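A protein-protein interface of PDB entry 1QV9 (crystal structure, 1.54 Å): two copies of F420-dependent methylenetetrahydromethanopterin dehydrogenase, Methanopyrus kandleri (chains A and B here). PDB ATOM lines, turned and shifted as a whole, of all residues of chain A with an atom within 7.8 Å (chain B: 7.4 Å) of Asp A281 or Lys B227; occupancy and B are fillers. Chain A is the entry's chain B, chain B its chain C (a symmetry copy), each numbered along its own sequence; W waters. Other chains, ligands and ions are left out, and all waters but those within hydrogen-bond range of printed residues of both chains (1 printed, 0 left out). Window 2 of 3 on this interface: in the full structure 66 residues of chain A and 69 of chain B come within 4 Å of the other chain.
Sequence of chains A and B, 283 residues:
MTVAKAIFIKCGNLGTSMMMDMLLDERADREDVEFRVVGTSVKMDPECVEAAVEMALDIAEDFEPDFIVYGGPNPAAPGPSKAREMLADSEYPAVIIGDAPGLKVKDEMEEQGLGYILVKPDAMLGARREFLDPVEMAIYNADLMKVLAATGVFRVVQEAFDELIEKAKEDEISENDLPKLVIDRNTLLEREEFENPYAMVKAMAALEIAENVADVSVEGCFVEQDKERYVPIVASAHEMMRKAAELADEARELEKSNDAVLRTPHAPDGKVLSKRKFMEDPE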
ATOM      1  N   PRO A 265      -9.977 -18.402 -19.818  1.00  0.00           N
ATOM      2  CA  PRO A 265      -9.680 -18.486 -18.380  1.00  0.00           C
ATOM      3  C   PRO A 265     -10.187 -17.287 -17.602  1.00  0.00           C
ATOM      4  O   PRO A 265     -10.391 -16.239 -18.193  1.00  0.00           O
ATOM      5  CB  PRO A 265      -8.168 -18.553 -18.343  1.00  0.00           C
ATOM      6  CG  PRO A 265      -7.760 -17.698 -19.527  1.00  0.00           C
ATOM      7  CD  PRO A 265      -8.789 -18.025 -20.603  1.00  0.00           C
ATOM      8  N   LEU A 273     -11.366 -14.091 -19.781  1.00  0.00           N
ATOM      9  CA  LEU A 273     -10.476 -13.676 -20.840  1.00  0.00           C
ATOM     10  C   LEU A 273     -10.668 -14.662 -21.989  1.00  0.00           C
ATOM     11  O   LEU A 273     -11.422 -15.632 -21.863  1.00  0.00           O
ATOM     12  CB  LEU A 273      -9.022 -13.695 -20.361  1.00  0.00           C
ATOM     13  CG  LEU A 273      -8.736 -12.967 -19.041  1.00  0.00           C
ATOM     14  CD1 LEU A 273      -7.263 -13.142 -18.668  1.00  0.00           C
ATOM     15  CD2 LEU A 273      -9.108 -11.473 -19.190  1.00  0.00           C
ATOM     16  N   SER A 274      -9.995 -14.396 -23.095  1.00  0.00           N
ATOM     17  CA  SER A 274     -10.116 -15.259 -24.264  1.00  0.00           C
ATOM     18  C   SER A 274      -8.832 -15.258 -25.069  1.00  0.00           C
ATOM     19  O   SER A 274      -8.105 -14.270 -25.089  1.00  0.00           O
ATOM     20  CB  SER A 274     -11.270 -14.771 -25.149  1.00  0.00           C
ATOM     21  OG  SER A 274     -11.428 -15.559 -26.325  1.00  0.00           O
ATOM     22  N   LYS A 275      -8.552 -16.378 -25.736  1.00  0.00           N
ATOM     23  CA  LYS A 275      -7.381 -16.490 -26.595  1.00  0.00           C
ATOM     24  C   LYS A 275      -7.608 -17.695 -27.523  1.00  0.00           C
ATOM     25  O   LYS A 275      -8.424 -18.575 -27.213  1.00  0.00           O
ATOM     26  CB  LYS A 275      -6.104 -16.717 -25.782  1.00  0.00           C
ATOM     27  CG  LYS A 275      -6.125 -17.966 -24.871  1.00  0.00           C
ATOM     28  CD  LYS A 275      -4.778 -18.218 -24.197  1.00  0.00           C
ATOM     29  CE  LYS A 275      -3.760 -18.922 -25.133  1.00  0.00           C
ATOM     30  NZ  LYS A 275      -2.392 -19.007 -24.548  1.00  0.00           N
ATOM     31  N   ARG A 276      -6.878 -17.711 -28.630  1.00  0.00           N
ATOM     32  CA  ARG A 276      -6.955 -18.816 -29.593  1.00  0.00           C
ATOM     33  C   ARG A 276      -5.595 -19.420 -29.874  1.00  0.00           C
ATOM     34  O   ARG A 276      -5.450 -20.644 -29.892  1.00  0.00           O
ATOM     35  CB  ARG A 276      -7.530 -18.339 -30.912  1.00  0.00           C
ATOM     36  CG  ARG A 276      -9.005 -18.108 -30.867  1.00  0.00           C
ATOM     37  CD  ARG A 276      -9.721 -19.280 -31.501  1.00  0.00           C
ATOM     38  NE  ARG A 276     -11.146 -19.142 -31.288  1.00  0.00           N
ATOM     39  CZ  ARG A 276     -12.009 -20.134 -31.407  1.00  0.00           C
ATOM     40  NH1 ARG A 276     -13.300 -19.921 -31.174  1.00  0.00           N
ATOM     41  NH2 ARG A 276     -11.569 -21.335 -31.759  1.00  0.00           N
ATOM     42  N   LYS A 277      -4.599 -18.586 -30.132  1.00  0.00           N
ATOM     43  CA  LYS A 277      -3.262 -19.101 -30.440  1.00  0.00           C
ATOM     44  C   LYS A 277      -2.554 -19.537 -29.178  1.00  0.00           C
ATOM     45  O   LYS A 277      -2.661 -18.909 -28.121  1.00  0.00           O
ATOM     46  CB  LYS A 277      -2.421 -18.066 -31.184  1.00  0.00           C
ATOM     47  CG  LYS A 277      -2.911 -17.769 -32.601  1.00  0.00           C
ATOM     48  CD  LYS A 277      -1.832 -17.025 -33.384  1.00  0.00           C
ATOM     49  CE  LYS A 277      -2.135 -17.023 -34.880  1.00  0.00           C
ATOM     50  NZ  LYS A 277      -2.086 -18.406 -35.459  1.00  0.00           N
ATOM     51  N   PHE A 278      -1.784 -20.613 -29.283  1.00  0.00           N
ATOM     52  CA  PHE A 278      -1.136 -21.130 -28.110  1.00  0.00           C
ATOM     53  C   PHE A 278      -0.291 -20.128 -27.331  1.00  0.00           C
ATOM     54  O   PHE A 278      -0.351 -20.094 -26.101  1.00  0.00           O
ATOM     55  CB  PHE A 278      -0.274 -22.336 -28.510  1.00  0.00           C
ATOM     56  CG  PHE A 278       0.363 -23.051 -27.350  1.00  0.00           C
ATOM     57  CD1 PHE A 278       1.738 -22.969 -27.133  1.00  0.00           C
ATOM     58  CD2 PHE A 278      -0.416 -23.807 -26.473  1.00  0.00           C
ATOM     59  CE1 PHE A 278       2.332 -23.631 -26.053  1.00  0.00           C
ATOM     60  CE2 PHE A 278       0.165 -24.471 -25.383  1.00  0.00           C
ATOM     61  CZ  PHE A 278       1.537 -24.382 -25.176  1.00  0.00           C
ATOM     62  N   MET A 279       0.488 -19.330 -28.052  1.00  0.00           N
ATOM     63  CA  MET A 279       1.370 -18.371 -27.391  1.00  0.00           C
ATOM     64  C   MET A 279       0.785 -16.985 -27.200  1.00  0.00           C
ATOM     65  O   MET A 279       1.489 -16.067 -26.801  1.00  0.00           O
ATOM     66  CB  MET A 279       2.692 -18.262 -28.148  1.00  0.00           C
ATOM     67  CG  MET A 279       3.440 -19.583 -28.296  1.00  0.00           C
ATOM     68  SD  MET A 279       4.184 -20.420 -26.668  1.00  0.00           S
ATOM     69  CE  MET A 279       3.349 -19.473 -25.311  1.00  0.00           C
ATOM     70  N   GLU A 280      -0.500 -16.852 -27.459  1.00  0.00           N
ATOM     71  CA  GLU A 280      -1.224 -15.586 -27.335  1.00  0.00           C
ATOM     72  C   GLU A 280      -1.678 -15.358 -25.883  1.00  0.00           C
ATOM     73  O   GLU A 280      -2.263 -16.249 -25.265  1.00  0.00           O
ATOM     74  CB  GLU A 280      -2.428 -15.692 -28.259  1.00  0.00           C
ATOM     75  CG  GLU A 280      -3.218 -14.463 -28.545  1.00  0.00           C
ATOM     76  CD  GLU A 280      -4.238 -14.743 -29.635  1.00  0.00           C
ATOM     77  OE1 GLU A 280      -5.132 -15.599 -29.419  1.00  0.00           O
ATOM     78  OE2 GLU A 280      -4.130 -14.120 -30.722  1.00  0.00           O
ATOM     79  N   ASP A 281      -1.398 -14.185 -25.316  1.00  0.00           N
ATOM     80  CA  ASP A 281      -1.851 -13.919 -23.952  1.00  0.00           C
ATOM     81  C   ASP A 281      -3.373 -13.783 -23.976  1.00  0.00           C
ATOM     82  O   ASP A 281      -3.935 -13.220 -24.918  1.00  0.00           O
ATOM     83  CB  ASP A 281      -1.263 -12.607 -23.398  1.00  0.00           C
ATOM     84  CG  ASP A 281       0.116 -12.785 -22.781  1.00  0.00           C
ATOM     85  OD1 ASP A 281       0.461 -13.911 -22.355  1.00  0.00           O
ATOM     86  OD2 ASP A 281       0.851 -11.777 -22.700  1.00  0.00           O
ATOM     87  N   PRO A 282      -4.061 -14.310 -22.953  1.00  0.00           N
ATOM     88  CA  PRO A 282      -5.524 -14.209 -22.903  1.00  0.00           C
ATOM     89  C   PRO A 282      -5.932 -12.787 -22.495  1.00  0.00           C
ATOM     90  O   PRO A 282      -5.406 -12.245 -21.516  1.00  0.00           O
ATOM     91  CB  PRO A 282      -5.910 -15.246 -21.858  1.00  0.00           C
ATOM     92  CG  PRO A 282      -4.703 -15.288 -20.958  1.00  0.00           C
ATOM     93  CD  PRO A 282      -3.547 -15.190 -21.887  1.00  0.00           C
ATOM     94  N   GLU A 283      -6.860 -12.199 -23.243  1.00  0.00           N
ATOM     95  CA  GLU A 283      -7.320 -10.838 -22.967  1.00  0.00           C
ATOM     96  C   GLU A 283      -8.783 -10.840 -22.547  1.00  0.00           C
ATOM     97  O   GLU A 283      -9.112 -10.116 -21.606  1.00  0.00           O
ATOM     98  CB  GLU A 283      -7.173  -9.950 -24.210  1.00  0.00           C
ATOM     99  CG  GLU A 283      -5.834 -10.028 -24.928  1.00  0.00           C
ATOM    100  CD  GLU A 283      -4.677  -9.533 -24.088  1.00  0.00           C
ATOM    101  OE1 GLU A 283      -4.444 -10.105 -23.002  1.00  0.00           O
ATOM    102  OE2 GLU A 283      -3.999  -8.572 -24.515  1.00  0.00           O
ATOM    103  OXT GLU A 283      -9.577 -11.421 -23.222  1.00  0.00           O
ATOM    104  N   ARG B 128      -1.429 -22.753 -15.163  1.00  0.00           N
ATOM    105  CA  ARG B 128      -0.950 -21.427 -15.564  1.00  0.00           C
ATOM    106  C   ARG B 128      -2.117 -20.808 -16.323  1.00  0.00           C
ATOM    107  O   ARG B 128      -2.721 -21.443 -17.198  1.00  0.00           O
ATOM    108  CB  ARG B 128       0.278 -21.511 -16.462  1.00  0.00           C
ATOM    109  CG  ARG B 128       1.582 -21.695 -15.730  1.00  0.00           C
ATOM    110  CD  ARG B 128       2.048 -20.409 -15.028  1.00  0.00           C
ATOM    111  NE  ARG B 128       3.434 -20.491 -14.592  1.00  0.00           N
ATOM    112  CZ  ARG B 128       4.122 -19.443 -14.133  1.00  0.00           C
ATOM    113  NH1 ARG B 128       5.375 -19.570 -13.746  1.00  0.00           N
ATOM    114  NH2 ARG B 128       3.539 -18.251 -14.079  1.00  0.00           N
ATOM    115  N   GLU B 130      -2.418 -18.837 -18.770  1.00  0.00           N
ATOM    116  CA  GLU B 130      -2.319 -18.779 -20.204  1.00  0.00           C
ATOM    117  C   GLU B 130      -2.702 -20.079 -20.884  1.00  0.00           C
ATOM    118  O   GLU B 130      -2.898 -20.124 -22.108  1.00  0.00           O
ATOM    119  CB  GLU B 130      -0.899 -18.430 -20.611  1.00  0.00           C
ATOM    120  CG  GLU B 130      -0.425 -17.074 -20.084  1.00  0.00           C
ATOM    121  CD  GLU B 130       0.370 -17.184 -18.810  1.00  0.00           C
ATOM    122  OE1 GLU B 130       1.273 -16.332 -18.612  1.00  0.00           O
ATOM    123  OE2 GLU B 130       0.112 -18.086 -17.983  1.00  0.00           O
ATOM    124  N   GLU B 224       9.889 -22.169 -13.528  1.00  0.00           N
ATOM    125  CA  GLU B 224      10.098 -21.378 -14.740  1.00  0.00           C
ATOM    126  C   GLU B 224       9.272 -20.100 -14.694  1.00  0.00           C
ATOM    127  O   GLU B 224       8.067 -20.151 -14.432  1.00  0.00           O
ATOM    128  CB  GLU B 224       9.716 -22.216 -15.973  1.00  0.00           C
ATOM    129  CG  GLU B 224       9.921 -21.495 -17.293  1.00  0.00           C
ATOM    130  CD  GLU B 224      11.353 -21.009 -17.494  1.00  0.00           C
ATOM    131  OE1 GLU B 224      11.579 -19.772 -17.448  1.00  0.00           O
ATOM    132  OE2 GLU B 224      12.254 -21.859 -17.701  1.00  0.00           O
ATOM    133  N   GLN B 225       9.926 -18.961 -14.935  1.00  0.00           N
ATOM    134  CA  GLN B 225       9.275 -17.659 -14.893  1.00  0.00           C
ATOM    135  C   GLN B 225       9.084 -16.978 -16.248  1.00  0.00           C
ATOM    136  O   GLN B 225       8.373 -15.966 -16.349  1.00  0.00           O
ATOM    137  CB  GLN B 225      10.075 -16.730 -13.969  1.00  0.00           C
ATOM    138  CG  GLN B 225      10.215 -17.253 -12.540  1.00  0.00           C
ATOM    139  CD  GLN B 225       8.881 -17.377 -11.844  1.00  0.00           C
ATOM    140  OE1 GLN B 225       8.122 -16.408 -11.763  1.00  0.00           O
ATOM    141  NE2 GLN B 225       8.579 -18.569 -11.337  1.00  0.00           N
ATOM    142  N   ASP B 226       9.723 -17.501 -17.290  1.00  0.00           N
ATOM    143  CA  ASP B 226       9.578 -16.938 -18.632  1.00  0.00           C
ATOM    144  C   ASP B 226       8.361 -17.619 -19.293  1.00  0.00           C
ATOM    145  O   ASP B 226       8.392 -18.825 -19.524  1.00  0.00           O
ATOM    146  CB  ASP B 226      10.866 -17.211 -19.436  1.00  0.00           C
ATOM    147  CG  ASP B 226      10.783 -16.711 -20.868  1.00  0.00           C
ATOM    148  OD1 ASP B 226      11.785 -16.817 -21.615  1.00  0.00           O
ATOM    149  OD2 ASP B 226       9.717 -16.204 -21.258  1.00  0.00           O
ATOM    150  N   LYS B 227       7.293 -16.872 -19.571  1.00  0.00           N
ATOM    151  CA  LYS B 227       6.082 -17.433 -20.199  1.00  0.00           C
ATOM    152  C   LYS B 227       6.367 -18.159 -21.514  1.00  0.00           C
ATOM    153  O   LYS B 227       5.596 -19.051 -21.900  1.00  0.00           O
ATOM    154  CB  LYS B 227       5.055 -16.341 -20.525  1.00  0.00           C
ATOM    155  CG  LYS B 227       5.408 -15.559 -21.805  1.00  0.00           C
ATOM    156  CD  LYS B 227       4.327 -14.549 -22.237  1.00  0.00           C
ATOM    157  CE  LYS B 227       3.604 -13.948 -21.047  1.00  0.00           C
ATOM    158  NZ  LYS B 227       2.807 -12.724 -21.411  1.00  0.00           N
ATOM    159  N   GLU B 228       7.421 -17.765 -22.230  1.00  0.00           N
ATOM    160  CA  GLU B 228       7.720 -18.423 -23.500  1.00  0.00           C
ATOM    161  C   GLU B 228       8.185 -19.855 -23.282  1.00  0.00           C
ATOM    162  O   GLU B 228       8.200 -20.678 -24.219  1.00  0.00           O
ATOM    163  CB  GLU B 228       8.775 -17.644 -24.282  1.00  0.00           C
ATOM    164  CG  GLU B 228       8.233 -16.341 -24.854  1.00  0.00           C
ATOM    165  CD  GLU B 228       9.127 -15.761 -25.934  1.00  0.00           C
ATOM    166  OE1 GLU B 228       8.659 -14.860 -26.665  1.00  0.00           O
ATOM    167  OE2 GLU B 228      10.296 -16.201 -26.053  1.00  0.00           O
ATOM    168  N   ARG B 229       8.572 -20.142 -22.048  1.00  0.00           N
ATOM    169  CA  ARG B 229       9.031 -21.483 -21.698  1.00  0.00           C
ATOM    170  C   ARG B 229       7.977 -22.182 -20.827  1.00  0.00           C
ATOM    171  O   ARG B 229       7.631 -23.330 -21.083  1.00  0.00           O
ATOM    172  CB  ARG B 229      10.368 -21.421 -20.951  1.00  0.00           C
ATOM    173  CG  ARG B 229      11.557 -20.998 -21.829  1.00  0.00           C
ATOM    174  CD  ARG B 229      12.786 -20.736 -20.947  1.00  0.00           C
ATOM    175  NE  ARG B 229      13.322 -21.973 -20.380  1.00  0.00           N
ATOM    176  CZ  ARG B 229      14.165 -22.769 -21.034  1.00  0.00           C
ATOM    177  NH1 ARG B 229      14.605 -23.889 -20.453  1.00  0.00           N
ATOM    178  NH2 ARG B 229      14.583 -22.437 -22.258  1.00  0.00           N
ATOM    179  N   TYR B 230       7.406 -21.503 -19.830  1.00  0.00           N
ATOM    180  CA  TYR B 230       6.433 -22.214 -18.993  1.00  0.00           C
ATOM    181  C   TYR B 230       5.087 -22.611 -19.615  1.00  0.00           C
ATOM    182  O   TYR B 230       4.490 -23.586 -19.149  1.00  0.00           O
ATOM    183  CB  TYR B 230       6.189 -21.521 -17.619  1.00  0.00           C
ATOM    184  CG  TYR B 230       5.467 -20.191 -17.596  1.00  0.00           C
ATOM    185  CD1 TYR B 230       6.126 -19.029 -17.155  1.00  0.00           C
ATOM    186  CD2 TYR B 230       4.132 -20.092 -17.935  1.00  0.00           C
ATOM    187  CE1 TYR B 230       5.446 -17.805 -17.060  1.00  0.00           C
ATOM    188  CE2 TYR B 230       3.442 -18.880 -17.842  1.00  0.00           C
ATOM    189  CZ  TYR B 230       4.114 -17.740 -17.402  1.00  0.00           C
ATOM    190  OH  TYR B 230       3.443 -16.534 -17.303  1.00  0.00           O
ATOM    191  N   VAL B 231       4.591 -21.889 -20.629  1.00  0.00           N
ATOM    192  CA  VAL B 231       3.311 -22.283 -21.234  1.00  0.00           C
ATOM    193  C   VAL B 231       3.570 -23.634 -21.967  1.00  0.00           C
ATOM    194  O   VAL B 231       2.802 -24.560 -21.795  1.00  0.00           O
ATOM    195  CB  VAL B 231       2.759 -21.181 -22.163  1.00  0.00           C
ATOM    196  CG1 VAL B 231       1.519 -21.640 -22.876  1.00  0.00           C
ATOM    197  CG2 VAL B 231       2.425 -19.951 -21.309  1.00  0.00           C
ATOM    198  N   PRO B 232       4.642 -23.733 -22.776  1.00  0.00           N
ATOM    199  CA  PRO B 232       4.896 -25.029 -23.432  1.00  0.00           C
ATOM    200  C   PRO B 232       5.127 -26.128 -22.382  1.00  0.00           C
ATOM    201  O   PRO B 232       4.671 -27.274 -22.543  1.00  0.00           O
ATOM    202  CB  PRO B 232       6.160 -24.774 -24.234  1.00  0.00           C
ATOM    203  CG  PRO B 232       6.018 -23.348 -24.632  1.00  0.00           C
ATOM    204  CD  PRO B 232       5.394 -22.655 -23.453  1.00  0.00           C
ATOM    205  N   ILE B 233       5.823 -25.809 -21.296  1.00  0.00           N
ATOM    206  CA  ILE B 233       6.081 -26.817 -20.282  1.00  0.00           C
ATOM    207  C   ILE B 233       4.794 -27.344 -19.675  1.00  0.00           C
ATOM    208  O   ILE B 233       4.602 -28.547 -19.593  1.00  0.00           O
ATOM    209  CB  ILE B 233       7.046 -26.263 -19.181  1.00  0.00           C
ATOM    210  CG1 ILE B 233       8.444 -26.117 -19.781  1.00  0.00           C
ATOM    211  CG2 ILE B 233       7.058 -27.175 -17.979  1.00  0.00           C
ATOM    212  CD1 ILE B 233       9.463 -25.371 -18.874  1.00  0.00           C
HETATM  213  O   HOH W   1       0.654 -13.861 -19.562  1.00  0.00           O
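Hydrophobic or aromatic side chains of chain B within 4 Å of the printed part of chain A: Val B231 and Pro B232.
Of the 12 printed residues of chain A, 4 touch a printed residue of chain B.
Printed residues of chain A that touch a printed residue of chain B: Lys A275, Phe A278, Met A279 and Asp A281.
Among the printed residues, 6 pairs touch across the chains.
Among the printed residues, Asp or Glu carboxylates within 4 Å of a Lys or Arg side-chain nitrogen of the other chain: Asp A281 with Lys B227 (2.5 Å).
The side-chain amino group of Lys A275 lies within hydrogen-bond range of the backbone carbonyl oxygen of Glu B130, at 2.7 Å.
The side-chain carboxylate of Asp A281 is in salt-bridge range of the side-chain amino group of Lys B227, at 2.5 Å.
Pro A265 touches none of the printed residues of chain B.
Of the printed residues of chain B, Lys A275 touches Glu B130 (2.7 Å).
Of the printed residues of chain B, Phe A278 touches Val B231 and Pro B232.
Printed residues of chain B within 4 Å of Asp A281: Glu B130 and Lys B227.
Of the printed residues of chain A, Glu B130 touches Lys A275 and Asp A281.
Glu B224 touches none of the printed residues of chain A.
Printed residues of chain A within 4 Å of Lys B227: Asp A281 (2.5 Å).
Of the printed residues of chain A, Val B231 touches Phe A278 and Met A279.
The nearest printed residue of chain B that does not touch Asp A281 is Tyr B230 (6.4 Å).
The nearest residue of chain A that does not touch Lys B227 is Met A279 (4.1 Å).
The nearest printed residue of chain A that does not touch Val B231 is Lys A275 (5.0 Å).
No position is printed for both chains.
Of the 6 pairs that touch across the chains among the printed residues, none has its exchanged pair printed and touching as well.
Water W1 lies within hydrogen-bond range of the side-chain carboxylate of Glu B130, the side-chain carboxylate of Asp A281 and the side-chain amino group of Lys B227.
Phe A278 touches Val B231 (CZ to CG1, 3.6 Å).
Phe A278 touches Pro B232 (CZ to CA, 3.8 Å).
CE of Met A279 touches CB of Val B231, at 3.6 Å.
CG of Glu B130 touches OD1 of Asp A281, 3.99 Å away.
The side-chain amino group of Lys A275 lies within hydrogen-bond range of the backbone carbonyl oxygen of Glu A280, 2.9 Å away.
OE1 of Glu B130 sits at hydrogen-bond distance from OH of Tyr B230 (2.5 Å).
The side-chain amino group (NZ) of Lys A275 lies within hydrogen-bond range of the backbone carbonyl oxygen (O) of Phe A278 (2.8 Å).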
